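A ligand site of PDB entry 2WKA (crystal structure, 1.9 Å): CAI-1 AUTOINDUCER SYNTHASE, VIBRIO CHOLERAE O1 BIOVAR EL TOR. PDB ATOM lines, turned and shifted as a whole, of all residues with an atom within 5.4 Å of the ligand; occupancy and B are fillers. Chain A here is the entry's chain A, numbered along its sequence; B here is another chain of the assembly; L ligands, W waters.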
ATOM      1  N   HIS A  30      36.223  -6.256 -13.630  1.00  0.00           N
ATOM      2  CA  HIS A  30      35.247  -7.272 -13.956  1.00  0.00           C
ATOM      3  C   HIS A  30      34.443  -6.784 -15.149  1.00  0.00           C
ATOM      4  O   HIS A  30      34.207  -5.596 -15.298  1.00  0.00           O
ATOM      5  CB  HIS A  30      34.304  -7.538 -12.772  1.00  0.00           C
ATOM      6  CG  HIS A  30      33.377  -8.697 -13.004  1.00  0.00           C
ATOM      7  ND1 HIS A  30      32.233  -8.583 -13.774  1.00  0.00           N
ATOM      8  CD2 HIS A  30      33.435  -9.981 -12.597  1.00  0.00           C
ATOM      9  CE1 HIS A  30      31.631  -9.754 -13.813  1.00  0.00           C
ATOM     10  NE2 HIS A  30      32.335 -10.620 -13.108  1.00  0.00           N
ATOM     11  N   VAL A  32      31.427  -6.589 -15.913  1.00  0.00           N
ATOM     12  CA  VAL A  32      30.221  -5.781 -15.722  1.00  0.00           C
ATOM     13  C   VAL A  32      30.555  -4.319 -15.503  1.00  0.00           C
ATOM     14  O   VAL A  32      29.655  -3.474 -15.490  1.00  0.00           O
ATOM     15  CB  VAL A  32      29.342  -6.291 -14.554  1.00  0.00           C
ATOM     16  CG1 VAL A  32      28.832  -7.691 -14.838  1.00  0.00           C
ATOM     17  CG2 VAL A  32      30.122  -6.235 -13.244  1.00  0.00           C
ATOM     18  N   SER A 107      13.652  -9.248   0.784  1.00  0.00           N
ATOM     19  CA  SER A 107      14.114  -9.161  -0.586  1.00  0.00           C
ATOM     20  C   SER A 107      13.332 -10.155  -1.415  1.00  0.00           C
ATOM     21  O   SER A 107      12.747 -11.092  -0.861  1.00  0.00           O
ATOM     22  CB  SER A 107      15.610  -9.497  -0.677  1.00  0.00           C
ATOM     23  OG  SER A 107      15.871 -10.825  -0.218  1.00  0.00           O
ATOM     24  N   GLY A 108      13.300  -9.963  -2.731  1.00  0.00           N
ATOM     25  CA  GLY A 108      12.688 -10.939  -3.625  1.00  0.00           C
ATOM     26  C   GLY A 108      13.392 -12.281  -3.530  1.00  0.00           C
ATOM     27  O   GLY A 108      12.760 -13.351  -3.663  1.00  0.00           O
ATOM     28  N   TRP A 109      14.716 -12.232  -3.330  1.00  0.00           N
ATOM     29  CA  TRP A 109      15.520 -13.441  -3.192  1.00  0.00           C
ATOM     30  C   TRP A 109      14.991 -14.266  -1.999  1.00  0.00           C
ATOM     31  O   TRP A 109      14.673 -15.448  -2.139  1.00  0.00           O
ATOM     32  CB  TRP A 109      17.008 -13.102  -3.001  1.00  0.00           C
ATOM     33  CG  TRP A 109      17.876 -14.314  -2.738  1.00  0.00           C
ATOM     34  CD1 TRP A 109      17.961 -15.012  -1.576  1.00  0.00           C
ATOM     35  CD2 TRP A 109      18.715 -14.992  -3.682  1.00  0.00           C
ATOM     36  NE1 TRP A 109      18.803 -16.085  -1.734  1.00  0.00           N
ATOM     37  CE2 TRP A 109      19.295 -16.090  -3.010  1.00  0.00           C
ATOM     38  CE3 TRP A 109      19.053 -14.766  -5.029  1.00  0.00           C
ATOM     39  CZ2 TRP A 109      20.190 -16.970  -3.640  1.00  0.00           C
ATOM     40  CZ3 TRP A 109      19.935 -15.645  -5.641  1.00  0.00           C
ATOM     41  CH2 TRP A 109      20.493 -16.731  -4.947  1.00  0.00           C
ATOM     42  N   ASN A 110      14.865 -13.626  -0.849  1.00  0.00           N
ATOM     43  CA  ASN A 110      14.385 -14.315   0.333  1.00  0.00           C
ATOM     44  C   ASN A 110      12.938 -14.796   0.197  1.00  0.00           C
ATOM     45  O   ASN A 110      12.584 -15.829   0.776  1.00  0.00           O
ATOM     46  CB  ASN A 110      14.557 -13.465   1.596  1.00  0.00           C
ATOM     47  CG  ASN A 110      16.029 -13.255   1.971  1.00  0.00           C
ATOM     48  OD1 ASN A 110      16.926 -13.704   1.262  1.00  0.00           O
ATOM     49  ND2 ASN A 110      16.251 -12.550   3.068  1.00  0.00           N
ATOM     50  N   ASN A 112      11.519 -15.922  -2.570  1.00  0.00           N
ATOM     51  CA  ASN A 112      11.564 -17.154  -3.335  1.00  0.00           C
ATOM     52  C   ASN A 112      12.161 -18.342  -2.551  1.00  0.00           C
ATOM     53  O   ASN A 112      11.602 -19.466  -2.554  1.00  0.00           O
ATOM     54  CB  ASN A 112      12.360 -16.909  -4.625  1.00  0.00           C
ATOM     55  CG  ASN A 112      11.544 -16.179  -5.681  1.00  0.00           C
ATOM     56  OD1 ASN A 112      10.303 -16.171  -5.641  1.00  0.00           O
ATOM     57  ND2 ASN A 112      12.229 -15.593  -6.646  1.00  0.00           N
ATOM     58  N   HIS A 133      14.615 -17.250 -12.457  1.00  0.00           N
ATOM     59  CA  HIS A 133      15.612 -16.512 -11.700  1.00  0.00           C
ATOM     60  C   HIS A 133      16.455 -17.407 -10.809  1.00  0.00           C
ATOM     61  O   HIS A 133      15.982 -18.412 -10.313  1.00  0.00           O
ATOM     62  CB  HIS A 133      14.955 -15.397 -10.882  1.00  0.00           C
ATOM     63  CG  HIS A 133      15.944 -14.429 -10.306  1.00  0.00           C
ATOM     64  ND1 HIS A 133      16.328 -14.456  -8.986  1.00  0.00           N
ATOM     65  CD2 HIS A 133      16.632 -13.420 -10.889  1.00  0.00           C
ATOM     66  CE1 HIS A 133      17.210 -13.493  -8.770  1.00  0.00           C
ATOM     67  NE2 HIS A 133      17.409 -12.845  -9.900  1.00  0.00           N
ATOM     68  N   SER A 135      17.430 -17.200  -7.807  1.00  0.00           N
ATOM     69  CA  SER A 135      16.883 -17.412  -6.475  1.00  0.00           C
ATOM     70  C   SER A 135      15.904 -18.586  -6.433  1.00  0.00           C
ATOM     71  O   SER A 135      15.761 -19.249  -5.412  1.00  0.00           O
ATOM     72  CB  SER A 135      16.199 -16.127  -5.953  1.00  0.00           C
ATOM     73  OG  SER A 135      15.123 -15.737  -6.807  1.00  0.00           O
ATOM     74  N   ASP A 173       9.231 -17.297 -14.194  1.00  0.00           N
ATOM     75  CA  ASP A 173       9.133 -15.826 -14.114  1.00  0.00           C
ATOM     76  C   ASP A 173       7.937 -15.479 -14.998  1.00  0.00           C
ATOM     77  O   ASP A 173       7.719 -16.133 -16.028  1.00  0.00           O
ATOM     78  CB  ASP A 173      10.354 -15.135 -14.732  1.00  0.00           C
ATOM     79  CG  ASP A 173      11.638 -15.299 -13.923  1.00  0.00           C
ATOM     80  OD1 ASP A 173      11.704 -16.047 -12.921  1.00  0.00           O
ATOM     81  OD2 ASP A 173      12.630 -14.650 -14.323  1.00  0.00           O
ATOM     82  N   ILE A 175       7.673 -12.393 -16.394  1.00  0.00           N
ATOM     83  CA  ILE A 175       8.518 -11.769 -17.384  1.00  0.00           C
ATOM     84  C   ILE A 175       9.973 -12.049 -17.013  1.00  0.00           C
ATOM     85  O   ILE A 175      10.395 -11.768 -15.884  1.00  0.00           O
ATOM     86  CB  ILE A 175       8.278 -10.249 -17.477  1.00  0.00           C
ATOM     87  CG1 ILE A 175       6.878  -9.985 -18.044  1.00  0.00           C
ATOM     88  CG2 ILE A 175       9.347  -9.589 -18.343  1.00  0.00           C
ATOM     89  CD1 ILE A 175       6.494  -8.504 -18.064  1.00  0.00           C
ATOM     90  N   SER A 177      14.001 -12.138 -16.597  1.00  0.00           N
ATOM     91  CA  SER A 177      14.846 -11.031 -16.190  1.00  0.00           C
ATOM     92  C   SER A 177      15.972 -10.677 -17.162  1.00  0.00           C
ATOM     93  O   SER A 177      16.375  -9.532 -17.224  1.00  0.00           O
ATOM     94  CB  SER A 177      15.368 -11.226 -14.754  1.00  0.00           C
ATOM     95  OG  SER A 177      16.166 -12.384 -14.657  1.00  0.00           O
ATOM     96  N   ASP A 202       6.882 -15.819 -10.453  1.00  0.00           N
ATOM     97  CA  ASP A 202       7.646 -14.656  -9.991  1.00  0.00           C
ATOM     98  C   ASP A 202       7.317 -13.457 -10.891  1.00  0.00           C
ATOM     99  O   ASP A 202       7.733 -13.416 -12.058  1.00  0.00           O
ATOM    100  CB  ASP A 202       9.157 -14.973  -9.988  1.00  0.00           C
ATOM    101  CG  ASP A 202      10.019 -13.826  -9.465  1.00  0.00           C
ATOM    102  OD1 ASP A 202       9.657 -12.639  -9.617  1.00  0.00           O
ATOM    103  OD2 ASP A 202      11.104 -14.108  -8.894  1.00  0.00           O
ATOM    104  N   SER A 204       8.288 -10.294 -10.468  1.00  0.00           N
ATOM    105  CA  SER A 204       9.183  -9.152 -10.187  1.00  0.00           C
ATOM    106  C   SER A 204       9.191  -8.099 -11.308  1.00  0.00           C
ATOM    107  O   SER A 204       9.266  -6.889 -11.031  1.00  0.00           O
ATOM    108  CB  SER A 204      10.614  -9.631  -9.922  1.00  0.00           C
ATOM    109  OG  SER A 204      10.674 -10.478  -8.808  1.00  0.00           O
ATOM    110  N   HIS A 205       9.136  -8.556 -12.552  1.00  0.00           N
ATOM    111  CA  HIS A 205       9.251  -7.641 -13.687  1.00  0.00           C
ATOM    112  C   HIS A 205       7.921  -7.262 -14.354  1.00  0.00           C
ATOM    113  O   HIS A 205       7.894  -6.476 -15.308  1.00  0.00           O
ATOM    114  CB  HIS A 205      10.280  -8.162 -14.701  1.00  0.00           C
ATOM    115  CG  HIS A 205      11.637  -8.333 -14.120  1.00  0.00           C
ATOM    116  ND1 HIS A 205      12.523  -7.291 -13.972  1.00  0.00           N
ATOM    117  CD2 HIS A 205      12.261  -9.425 -13.605  1.00  0.00           C
ATOM    118  CE1 HIS A 205      13.633  -7.725 -13.396  1.00  0.00           C
ATOM    119  NE2 HIS A 205      13.500  -9.017 -13.161  1.00  0.00           N
ATOM    120  N   SER A 233      10.146  -9.398  -6.157  1.00  0.00           N
ATOM    121  CA  SER A 233      11.000  -8.370  -5.588  1.00  0.00           C
ATOM    122  C   SER A 233      10.231  -7.063  -5.562  1.00  0.00           C
ATOM    123  O   SER A 233       9.545  -6.722  -6.550  1.00  0.00           O
ATOM    124  CB  SER A 233      12.226  -8.143  -6.458  1.00  0.00           C
ATOM    125  OG  SER A 233      12.947  -7.026  -5.964  1.00  0.00           O
ATOM    126  N   LEU A 234      10.350  -6.301  -4.478  1.00  0.00           N
ATOM    127  CA  LEU A 234       9.787  -4.938  -4.477  1.00  0.00           C
ATOM    128  C   LEU A 234      10.872  -3.924  -4.836  1.00  0.00           C
ATOM    129  O   LEU A 234      10.677  -2.697  -4.713  1.00  0.00           O
ATOM    130  CB  LEU A 234       9.094  -4.608  -3.134  1.00  0.00           C
ATOM    131  CG  LEU A 234       7.959  -5.578  -2.725  1.00  0.00           C
ATOM    132  CD1 LEU A 234       7.454  -5.260  -1.322  1.00  0.00           C
ATOM    133  CD2 LEU A 234       6.797  -5.564  -3.714  1.00  0.00           C
ATOM    134  N   ALA A 235      11.992  -4.428  -5.368  1.00  0.00           N
ATOM    135  CA  ALA A 235      13.137  -3.590  -5.763  1.00  0.00           C
ATOM    136  C   ALA A 235      13.119  -3.169  -7.237  1.00  0.00           C
ATOM    137  O   ALA A 235      14.086  -2.599  -7.740  1.00  0.00           O
ATOM    138  CB  ALA A 235      14.463  -4.291  -5.429  1.00  0.00           C
ATOM    139  N   LYS A 236      12.016  -3.448  -7.916  1.00  0.00           N
ATOM    140  CA  LYS A 236      11.874  -3.078  -9.317  1.00  0.00           C
ATOM    141  C   LYS A 236      10.878  -1.936  -9.403  1.00  0.00           C
ATOM    142  O   LYS A 236      11.184  -0.822  -9.012  1.00  0.00           O
ATOM    143  CB  LYS A 236      11.449  -4.278 -10.167  1.00  0.00           C
ATOM    144  CG  LYS A 236      12.189  -5.601  -9.875  1.00  0.00           C
ATOM    145  CD  LYS A 236      13.685  -5.435  -9.817  1.00  0.00           C
ATOM    146  CE  LYS A 236      14.362  -6.794  -9.640  1.00  0.00           C
ATOM    147  NZ  LYS A 236      15.551  -6.660  -8.774  1.00  0.00           N
ATOM    148  N   ALA A 242      13.113  -5.012  -0.766  1.00  0.00           N
ATOM    149  CA  ALA A 242      12.210  -5.905  -0.047  1.00  0.00           C
ATOM    150  C   ALA A 242      11.594  -6.862  -1.039  1.00  0.00           C
ATOM    151  O   ALA A 242      11.895  -6.803  -2.237  1.00  0.00           O
ATOM    152  CB  ALA A 242      11.143  -5.132   0.680  1.00  0.00           C
ATOM    153  N   GLY A 243      10.743  -7.761  -0.549  1.00  0.00           N
ATOM    154  CA  GLY A 243      10.095  -8.755  -1.402  1.00  0.00           C
ATOM    155  C   GLY A 243       8.787  -9.149  -0.777  1.00  0.00           C
ATOM    156  O   GLY A 243       8.487  -8.738   0.333  1.00  0.00           O
ATOM    157  N   VAL A 344      25.701  -5.375 -18.518  1.00  0.00           N
ATOM    158  CA  VAL A 344      26.275  -6.652 -18.904  1.00  0.00           C
ATOM    159  C   VAL A 344      25.761  -7.782 -18.009  1.00  0.00           C
ATOM    160  O   VAL A 344      25.946  -7.765 -16.800  1.00  0.00           O
ATOM    161  CB  VAL A 344      27.809  -6.658 -18.770  1.00  0.00           C
ATOM    162  CG1 VAL A 344      28.317  -8.079 -18.935  1.00  0.00           C
ATOM    163  CG2 VAL A 344      28.451  -5.729 -19.781  1.00  0.00           C
ATOM    164  N   PHE A 345      25.108  -8.753 -18.612  1.00  0.00           N
ATOM    165  CA  PHE A 345      24.766  -9.966 -17.897  1.00  0.00           C
ATOM    166  C   PHE A 345      25.696 -11.078 -18.361  1.00  0.00           C
ATOM    167  O   PHE A 345      25.797 -11.375 -19.545  1.00  0.00           O
ATOM    168  CB  PHE A 345      23.293 -10.346 -18.120  1.00  0.00           C
ATOM    169  CG  PHE A 345      22.361  -9.721 -17.130  1.00  0.00           C
ATOM    170  CD1 PHE A 345      22.148  -8.353 -17.128  1.00  0.00           C
ATOM    171  CD2 PHE A 345      21.707 -10.500 -16.186  1.00  0.00           C
ATOM    172  CE1 PHE A 345      21.293  -7.774 -16.201  1.00  0.00           C
ATOM    173  CE2 PHE A 345      20.852  -9.921 -15.260  1.00  0.00           C
ATOM    174  CZ  PHE A 345      20.647  -8.564 -15.263  1.00  0.00           C
ATOM    175  N   CYS A 346      26.409 -11.672 -17.416  1.00  0.00           N
ATOM    176  CA  CYS A 346      27.412 -12.657 -17.756  1.00  0.00           C
ATOM    177  C   CYS A 346      27.363 -13.758 -16.728  1.00  0.00           C
ATOM    178  O   CYS A 346      26.443 -13.838 -15.921  1.00  0.00           O
ATOM    179  CB  CYS A 346      28.809 -12.034 -17.803  1.00  0.00           C
ATOM    180  SG  CYS A 346      29.333 -11.186 -16.272  1.00  0.00           S
ATOM    181  N   ARG A 347      28.351 -14.620 -16.764  1.00  0.00           N
ATOM    182  CA  ARG A 347      28.349 -15.746 -15.861  1.00  0.00           C
ATOM    183  C   ARG A 347      28.548 -15.367 -14.413  1.00  0.00           C
ATOM    184  O   ARG A 347      29.450 -14.586 -14.111  1.00  0.00           O
ATOM    185  CB  ARG A 347      29.481 -16.690 -16.221  1.00  0.00           C
ATOM    186  CG  ARG A 347      30.793 -16.216 -15.644  1.00  0.00           C
ATOM    187  CD  ARG A 347      31.945 -16.405 -16.599  1.00  0.00           C
ATOM    188  NE  ARG A 347      32.558 -17.710 -16.445  1.00  0.00           N
ATOM    189  CZ  ARG A 347      33.855 -17.932 -16.565  1.00  0.00           C
ATOM    190  NH1 ARG A 347      34.676 -16.929 -16.846  1.00  0.00           N
ATOM    191  NH2 ARG A 347      34.336 -19.158 -16.396  1.00  0.00           N
ATOM    192  N   PRO A 348      27.513 -15.619 -13.608  1.00  0.00           N
ATOM    193  CA  PRO A 348      27.121 -16.931 -13.151  1.00  0.00           C
ATOM    194  C   PRO A 348      25.648 -16.841 -13.551  1.00  0.00           C
ATOM    195  O   PRO A 348      24.891 -17.799 -13.437  1.00  0.00           O
ATOM    196  CB  PRO A 348      27.310 -16.892 -11.628  1.00  0.00           C
ATOM    197  CG  PRO A 348      27.310 -15.486 -11.263  1.00  0.00           C
ATOM    198  CD  PRO A 348      27.400 -14.640 -12.522  1.00  0.00           C
ATOM    199  N   ALA A 349      25.263 -15.665 -14.052  1.00  0.00           N
ATOM    200  CA  ALA A 349      23.877 -15.421 -14.480  1.00  0.00           C
ATOM    201  C   ALA A 349      23.574 -16.072 -15.827  1.00  0.00           C
ATOM    202  O   ALA A 349      22.483 -16.578 -16.035  1.00  0.00           O
ATOM    203  CB  ALA A 349      23.578 -13.926 -14.532  1.00  0.00           C
ATOM    204  N   SER B  76      21.856  -4.597  -8.846  1.00  0.00           N
ATOM    205  CA  SER B  76      22.861  -5.394  -8.136  1.00  0.00           C
ATOM    206  C   SER B  76      24.091  -4.545  -7.754  1.00  0.00           C
ATOM    207  O   SER B  76      24.516  -3.669  -8.521  1.00  0.00           O
ATOM    208  CB  SER B  76      23.271  -6.573  -9.009  1.00  0.00           C
ATOM    209  OG  SER B  76      24.514  -7.128  -8.617  1.00  0.00           O
ATOM    210  N   SER B  78      26.940  -5.597  -7.761  1.00  0.00           N
ATOM    211  CA  SER B  78      28.026  -6.021  -8.633  1.00  0.00           C
ATOM    212  C   SER B  78      28.406  -4.872  -9.571  1.00  0.00           C
ATOM    213  O   SER B  78      29.580  -4.646  -9.863  1.00  0.00           O
ATOM    214  CB  SER B  78      27.611  -7.262  -9.456  1.00  0.00           C
ATOM    215  OG  SER B  78      27.371  -8.381  -8.622  1.00  0.00           O
ATOM    216  N   PHE B  79      27.391  -4.123 -10.008  1.00  0.00           N
ATOM    217  CA  PHE B  79      27.570  -3.030 -10.957  1.00  0.00           C
ATOM    218  C   PHE B  79      28.101  -1.759 -10.283  1.00  0.00           C
ATOM    219  O   PHE B  79      28.440  -0.786 -10.970  1.00  0.00           O
ATOM    220  CB  PHE B  79      26.241  -2.702 -11.638  1.00  0.00           C
ATOM    221  CG  PHE B  79      25.663  -3.851 -12.441  1.00  0.00           C
ATOM    222  CD1 PHE B  79      26.304  -4.306 -13.581  1.00  0.00           C
ATOM    223  CD2 PHE B  79      24.473  -4.446 -12.061  1.00  0.00           C
ATOM    224  CE1 PHE B  79      25.778  -5.357 -14.319  1.00  0.00           C
ATOM    225  CE2 PHE B  79      23.939  -5.487 -12.795  1.00  0.00           C
ATOM    226  CZ  PHE B  79      24.594  -5.943 -13.930  1.00  0.00           C
ATOM    227  N   PRO B 256      31.922  -9.307  -4.270  1.00  0.00           N
ATOM    228  CA  PRO B 256      30.806  -8.674  -4.996  1.00  0.00           C
ATOM    229  C   PRO B 256      30.429  -9.369  -6.306  1.00  0.00           C
ATOM    230  O   PRO B 256      29.307  -9.184  -6.804  1.00  0.00           O
ATOM    231  CB  PRO B 256      31.320  -7.258  -5.276  1.00  0.00           C
ATOM    232  CG  PRO B 256      32.383  -7.024  -4.252  1.00  0.00           C
ATOM    233  CD  PRO B 256      33.026  -8.371  -4.034  1.00  0.00           C
ATOM    234  N   PHE B 257      31.345 -10.170  -6.843  1.00  0.00           N
ATOM    235  CA  PHE B 257      31.118 -10.836  -8.128  1.00  0.00           C
ATOM    236  C   PHE B 257      30.960 -12.337  -7.977  1.00  0.00           C
ATOM    237  O   PHE B 257      30.850 -13.049  -8.963  1.00  0.00           O
ATOM    238  CB  PHE B 257      32.302 -10.565  -9.064  1.00  0.00           C
ATOM    239  CG  PHE B 257      32.608  -9.115  -9.226  1.00  0.00           C
ATOM    240  CD1 PHE B 257      31.792  -8.301  -9.987  1.00  0.00           C
ATOM    241  CD2 PHE B 257      33.721  -8.556  -8.612  1.00  0.00           C
ATOM    242  CE1 PHE B 257      32.064  -6.958 -10.134  1.00  0.00           C
ATOM    243  CE2 PHE B 257      34.012  -7.204  -8.746  1.00  0.00           C
ATOM    244  CZ  PHE B 257      33.181  -6.410  -9.511  1.00  0.00           C
ATOM    245  N   ILE B 263      25.276 -10.608  -5.867  1.00  0.00           N
ATOM    246  CA  ILE B 263      25.003 -10.450  -7.297  1.00  0.00           C
ATOM    247  C   ILE B 263      23.511 -10.318  -7.630  1.00  0.00           C
ATOM    248  O   ILE B 263      23.103  -9.433  -8.396  1.00  0.00           O
ATOM    249  CB  ILE B 263      25.514 -11.675  -8.099  1.00  0.00           C
ATOM    250  CG1 ILE B 263      27.027 -11.860  -7.936  1.00  0.00           C
ATOM    251  CG2 ILE B 263      25.152 -11.551  -9.585  1.00  0.00           C
ATOM    252  CD1 ILE B 263      27.474 -13.298  -8.261  1.00  0.00           C
ATOM    253  N   PHE B 264      22.715 -11.210  -7.055  1.00  0.00           N
ATOM    254  CA  PHE B 264      21.353 -11.448  -7.521  1.00  0.00           C
ATOM    255  C   PHE B 264      20.249 -10.833  -6.645  1.00  0.00           C
ATOM    256  O   PHE B 264      19.065 -11.122  -6.867  1.00  0.00           O
ATOM    257  CB  PHE B 264      21.084 -12.954  -7.606  1.00  0.00           C
ATOM    258  CG  PHE B 264      21.888 -13.671  -8.656  1.00  0.00           C
ATOM    259  CD1 PHE B 264      21.556 -13.528 -10.000  1.00  0.00           C
ATOM    260  CD2 PHE B 264      22.951 -14.484  -8.314  1.00  0.00           C
ATOM    261  CE1 PHE B 264      22.267 -14.177 -10.978  1.00  0.00           C
ATOM    262  CE2 PHE B 264      23.679 -15.135  -9.301  1.00  0.00           C
ATOM    263  CZ  PHE B 264      23.316 -14.990 -10.640  1.00  0.00           C
ATOM    264  N   SER B 265      20.620 -10.039  -5.645  1.00  0.00           N
ATOM    265  CA  SER B 265      19.649  -9.382  -4.780  1.00  0.00           C
ATOM    266  C   SER B 265      20.014  -7.903  -4.700  1.00  0.00           C
ATOM    267  O   SER B 265      21.195  -7.555  -4.667  1.00  0.00           O
ATOM    268  CB  SER B 265      19.640 -10.042  -3.388  1.00  0.00           C
ATOM    269  OG  SER B 265      18.484  -9.694  -2.640  1.00  0.00           O
ATOM    270  N   SER B 266      19.003  -7.031  -4.709  1.00  0.00           N
ATOM    271  CA  SER B 266      19.260  -5.596  -4.834  1.00  0.00           C
ATOM    272  C   SER B 266      20.093  -5.014  -3.693  1.00  0.00           C
ATOM    273  O   SER B 266      20.035  -5.442  -2.540  1.00  0.00           O
ATOM    274  CB  SER B 266      17.961  -4.784  -5.022  1.00  0.00           C
ATOM    275  OG  SER B 266      17.338  -4.520  -3.773  1.00  0.00           O
HETATM  276  C1  LIG L   1      29.106 -11.104 -11.668  1.00  0.00           C
HETATM  277  C2  LIG L   1      27.983 -10.389 -12.443  1.00  0.00           C
HETATM  278  C3  LIG L   1      26.977 -11.406 -13.001  1.00  0.00           C
HETATM  279  C4  LIG L   1      26.046 -10.777 -14.046  1.00  0.00           C
HETATM  280  C5  LIG L   1      25.072  -9.732 -13.461  1.00  0.00           C
HETATM  281  C6  LIG L   1      23.859 -10.383 -12.790  1.00  0.00           C
HETATM  282  C7  LIG L   1      22.881  -9.338 -12.214  1.00  0.00           C
HETATM  283  C8  LIG L   1      21.634 -10.007 -11.605  1.00  0.00           C
HETATM  284  C9  LIG L   1      20.704  -8.994 -10.931  1.00  0.00           C
HETATM  285  C10 LIG L   1      19.403  -9.702 -10.531  1.00  0.00           C
HETATM  286  O1  LIG L   1      19.271 -10.907 -10.744  1.00  0.00           O
HETATM  287  C11 LIG L   1      18.231  -9.003  -9.887  1.00  0.00           C
HETATM  288  N1  LIG L   1      17.272  -9.906  -9.714  1.00  0.00           N
HETATM  289  C12 LIG L   1      16.137  -9.701  -9.103  1.00  0.00           C
HETATM  290  C13 LIG L   1      15.174 -10.716  -9.053  1.00  0.00           C
HETATM  291  C14 LIG L   1      14.536 -11.052 -10.242  1.00  0.00           C
HETATM  292  O2  LIG L   1      14.887 -10.424 -11.382  1.00  0.00           O
HETATM  293  C15 LIG L   1      13.532 -12.014 -10.238  1.00  0.00           C
HETATM  294  C16 LIG L   1      12.830 -12.416 -11.542  1.00  0.00           C
HETATM  295  N2  LIG L   1      13.202 -12.613  -9.085  1.00  0.00           N
HETATM  296  C17 LIG L   1      13.805 -12.305  -7.958  1.00  0.00           C
HETATM  297  C18 LIG L   1      14.806 -11.343  -7.882  1.00  0.00           C
HETATM  298  C19 LIG L   1      15.432 -11.055  -6.531  1.00  0.00           C
HETATM  299  O3  LIG L   1      14.856  -9.907  -5.979  1.00  0.00           O
HETATM  300  P1  LIG L   1      15.690  -8.975  -4.953  1.00  0.00           P
HETATM  301  O4  LIG L   1      16.355  -9.946  -3.871  1.00  0.00           O
HETATM  302  O5  LIG L   1      14.550  -8.147  -4.199  1.00  0.00           O
HETATM  303  O6  LIG L   1      16.737  -8.192  -5.659  1.00  0.00           O
HETATM  304  O   HOH W   1      19.103 -12.552 -13.571  1.00  0.00           O
HETATM  305  O   HOH W   2      15.537  -6.318  -2.394  1.00  0.00           O
HETATM  306  O   HOH W   3      17.141  -7.403 -12.476  1.00  0.00           O
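The side-chain hydroxyl of Ser 265 of chain B is in hydrogen-bond range of an oxygen (O4) of the ligand, at 2.5 Å.
N2 of the ligand lies within hydrogen-bond range of OD2 of Asp 202 (2.6 Å).
The side-chain hydroxyl (OG) of Ser 233 lies within hydrogen-bond range of an oxygen (O5) of the ligand (2.6 Å).
N of Gly 108 sits at hydrogen-bond distance from O5 of the ligand, at 2.6 Å.
A ring nitrogen (NE2) of His 205 sits at hydrogen-bond distance from an oxygen (O2) of the ligand (2.7 Å).
The backbone NH of Ser 266 of chain B lies within hydrogen-bond range of an oxygen (O6) of the ligand (2.7 Å).
O1 of the ligand sits at hydrogen-bond distance from NE2 of His 133, 2.8 Å away.
An oxygen (O4) of the ligand lies within hydrogen-bond range of the backbone NH (N) of Trp 109, 2.9 Å away.
The side-chain amino group of Lys 236 is in salt-bridge range of an oxygen (O6) of the ligand, 3.7 Å away.
The side-chain hydroxyl (OG) of Ser 204 lies within hydrogen-bond range of a nitrogen (N2) of the ligand (3.3 Å).
The side-chain carboxylate of Asp 202 lies within hydrogen-bond range of the side-chain hydroxyl of Ser 204 (2.5 Å).
The side-chain hydroxyl (OG) of Ser 204 lies within hydrogen-bond range of the backbone NH (N) of Ser 233, at 2.9 Å.
The side-chain hydroxyl (OG) of Ser 233 lies within hydrogen-bond range of the backbone NH (N) of Ala 235 (2.8 Å).
The backbone carbonyl oxygen (O) of Ala 242 is in hydrogen-bond range of the backbone NH (N) of Gly 108 (3.5 Å).
N of His 133 sits at hydrogen-bond distance from OD1 of Asp 173.
The backbone NH of Asn 110 sits at hydrogen-bond distance from the side-chain hydroxyl of Ser 107, 3.0 Å away.
The backbone carbonyl oxygen of Ile 263 of chain B sits at hydrogen-bond distance from the side-chain hydroxyl of Ser 76 of chain B, at 2.7 Å.
OG of Ser 135 sits at hydrogen-bond distance from ND2 of Asn 112 (2.9 Å).
His 30 touches the ligand (NE2 to C1, 3.6 Å).
Val 32 touches the ligand (CG1 to C2, 3.7 Å).
Ser 107 touches the ligand (CB to O4, 3.3 Å).
ND2 of Asn 112 touches C17 of the ligand, 3.9 Å away.
OG of Ser 135 touches C17 of the ligand (3.9 Å).
Asp 173 touches the ligand.
Ser 177 touches the ligand (CB to O2, 3.5 Å).
O of Ala 242 touches O5 of the ligand, at 3.6 Å.
Val 344 touches the ligand.
Phe 345 touches the ligand (CE2 to C7, 3.7 Å).
Cys 346 touches the ligand.
Pro 348 touches the ligand.
CB of Ala 349 touches C6 of the ligand, 3.96 Å away.
CZ of Phe 79 of chain B touches C5 of the ligand (3.8 Å).
Phe 257 of chain B touches the ligand (O to C1, 3.8 Å).
Ile 263 of chain B touches the ligand.
Phe 264 of chain B touches the ligand (CD1 to O1, 3.6 Å).
Hydrophobic or aromatic side chains within 4 Å of the ligand: His 30, Val 32, Trp 109, His 133, His 205, Phe 345, Pro 348, Ala 349, Phe 79 of chain B, Ile 263 of chain B and Phe 264 of chain B.
Of the 36 residues printed, 27 come within 4 Å of the ligand.
Water W2 lies within hydrogen-bond range of O5 of the ligand (2.8 Å), OG of Ser 266 of chain B (2.9 Å) and N of Ala 242 (3.2 Å).
Water W1 bridges the side-chain hydroxyl of Ser 177 (3.1 Å) and an oxygen (O1) of the ligand (3.3 Å).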
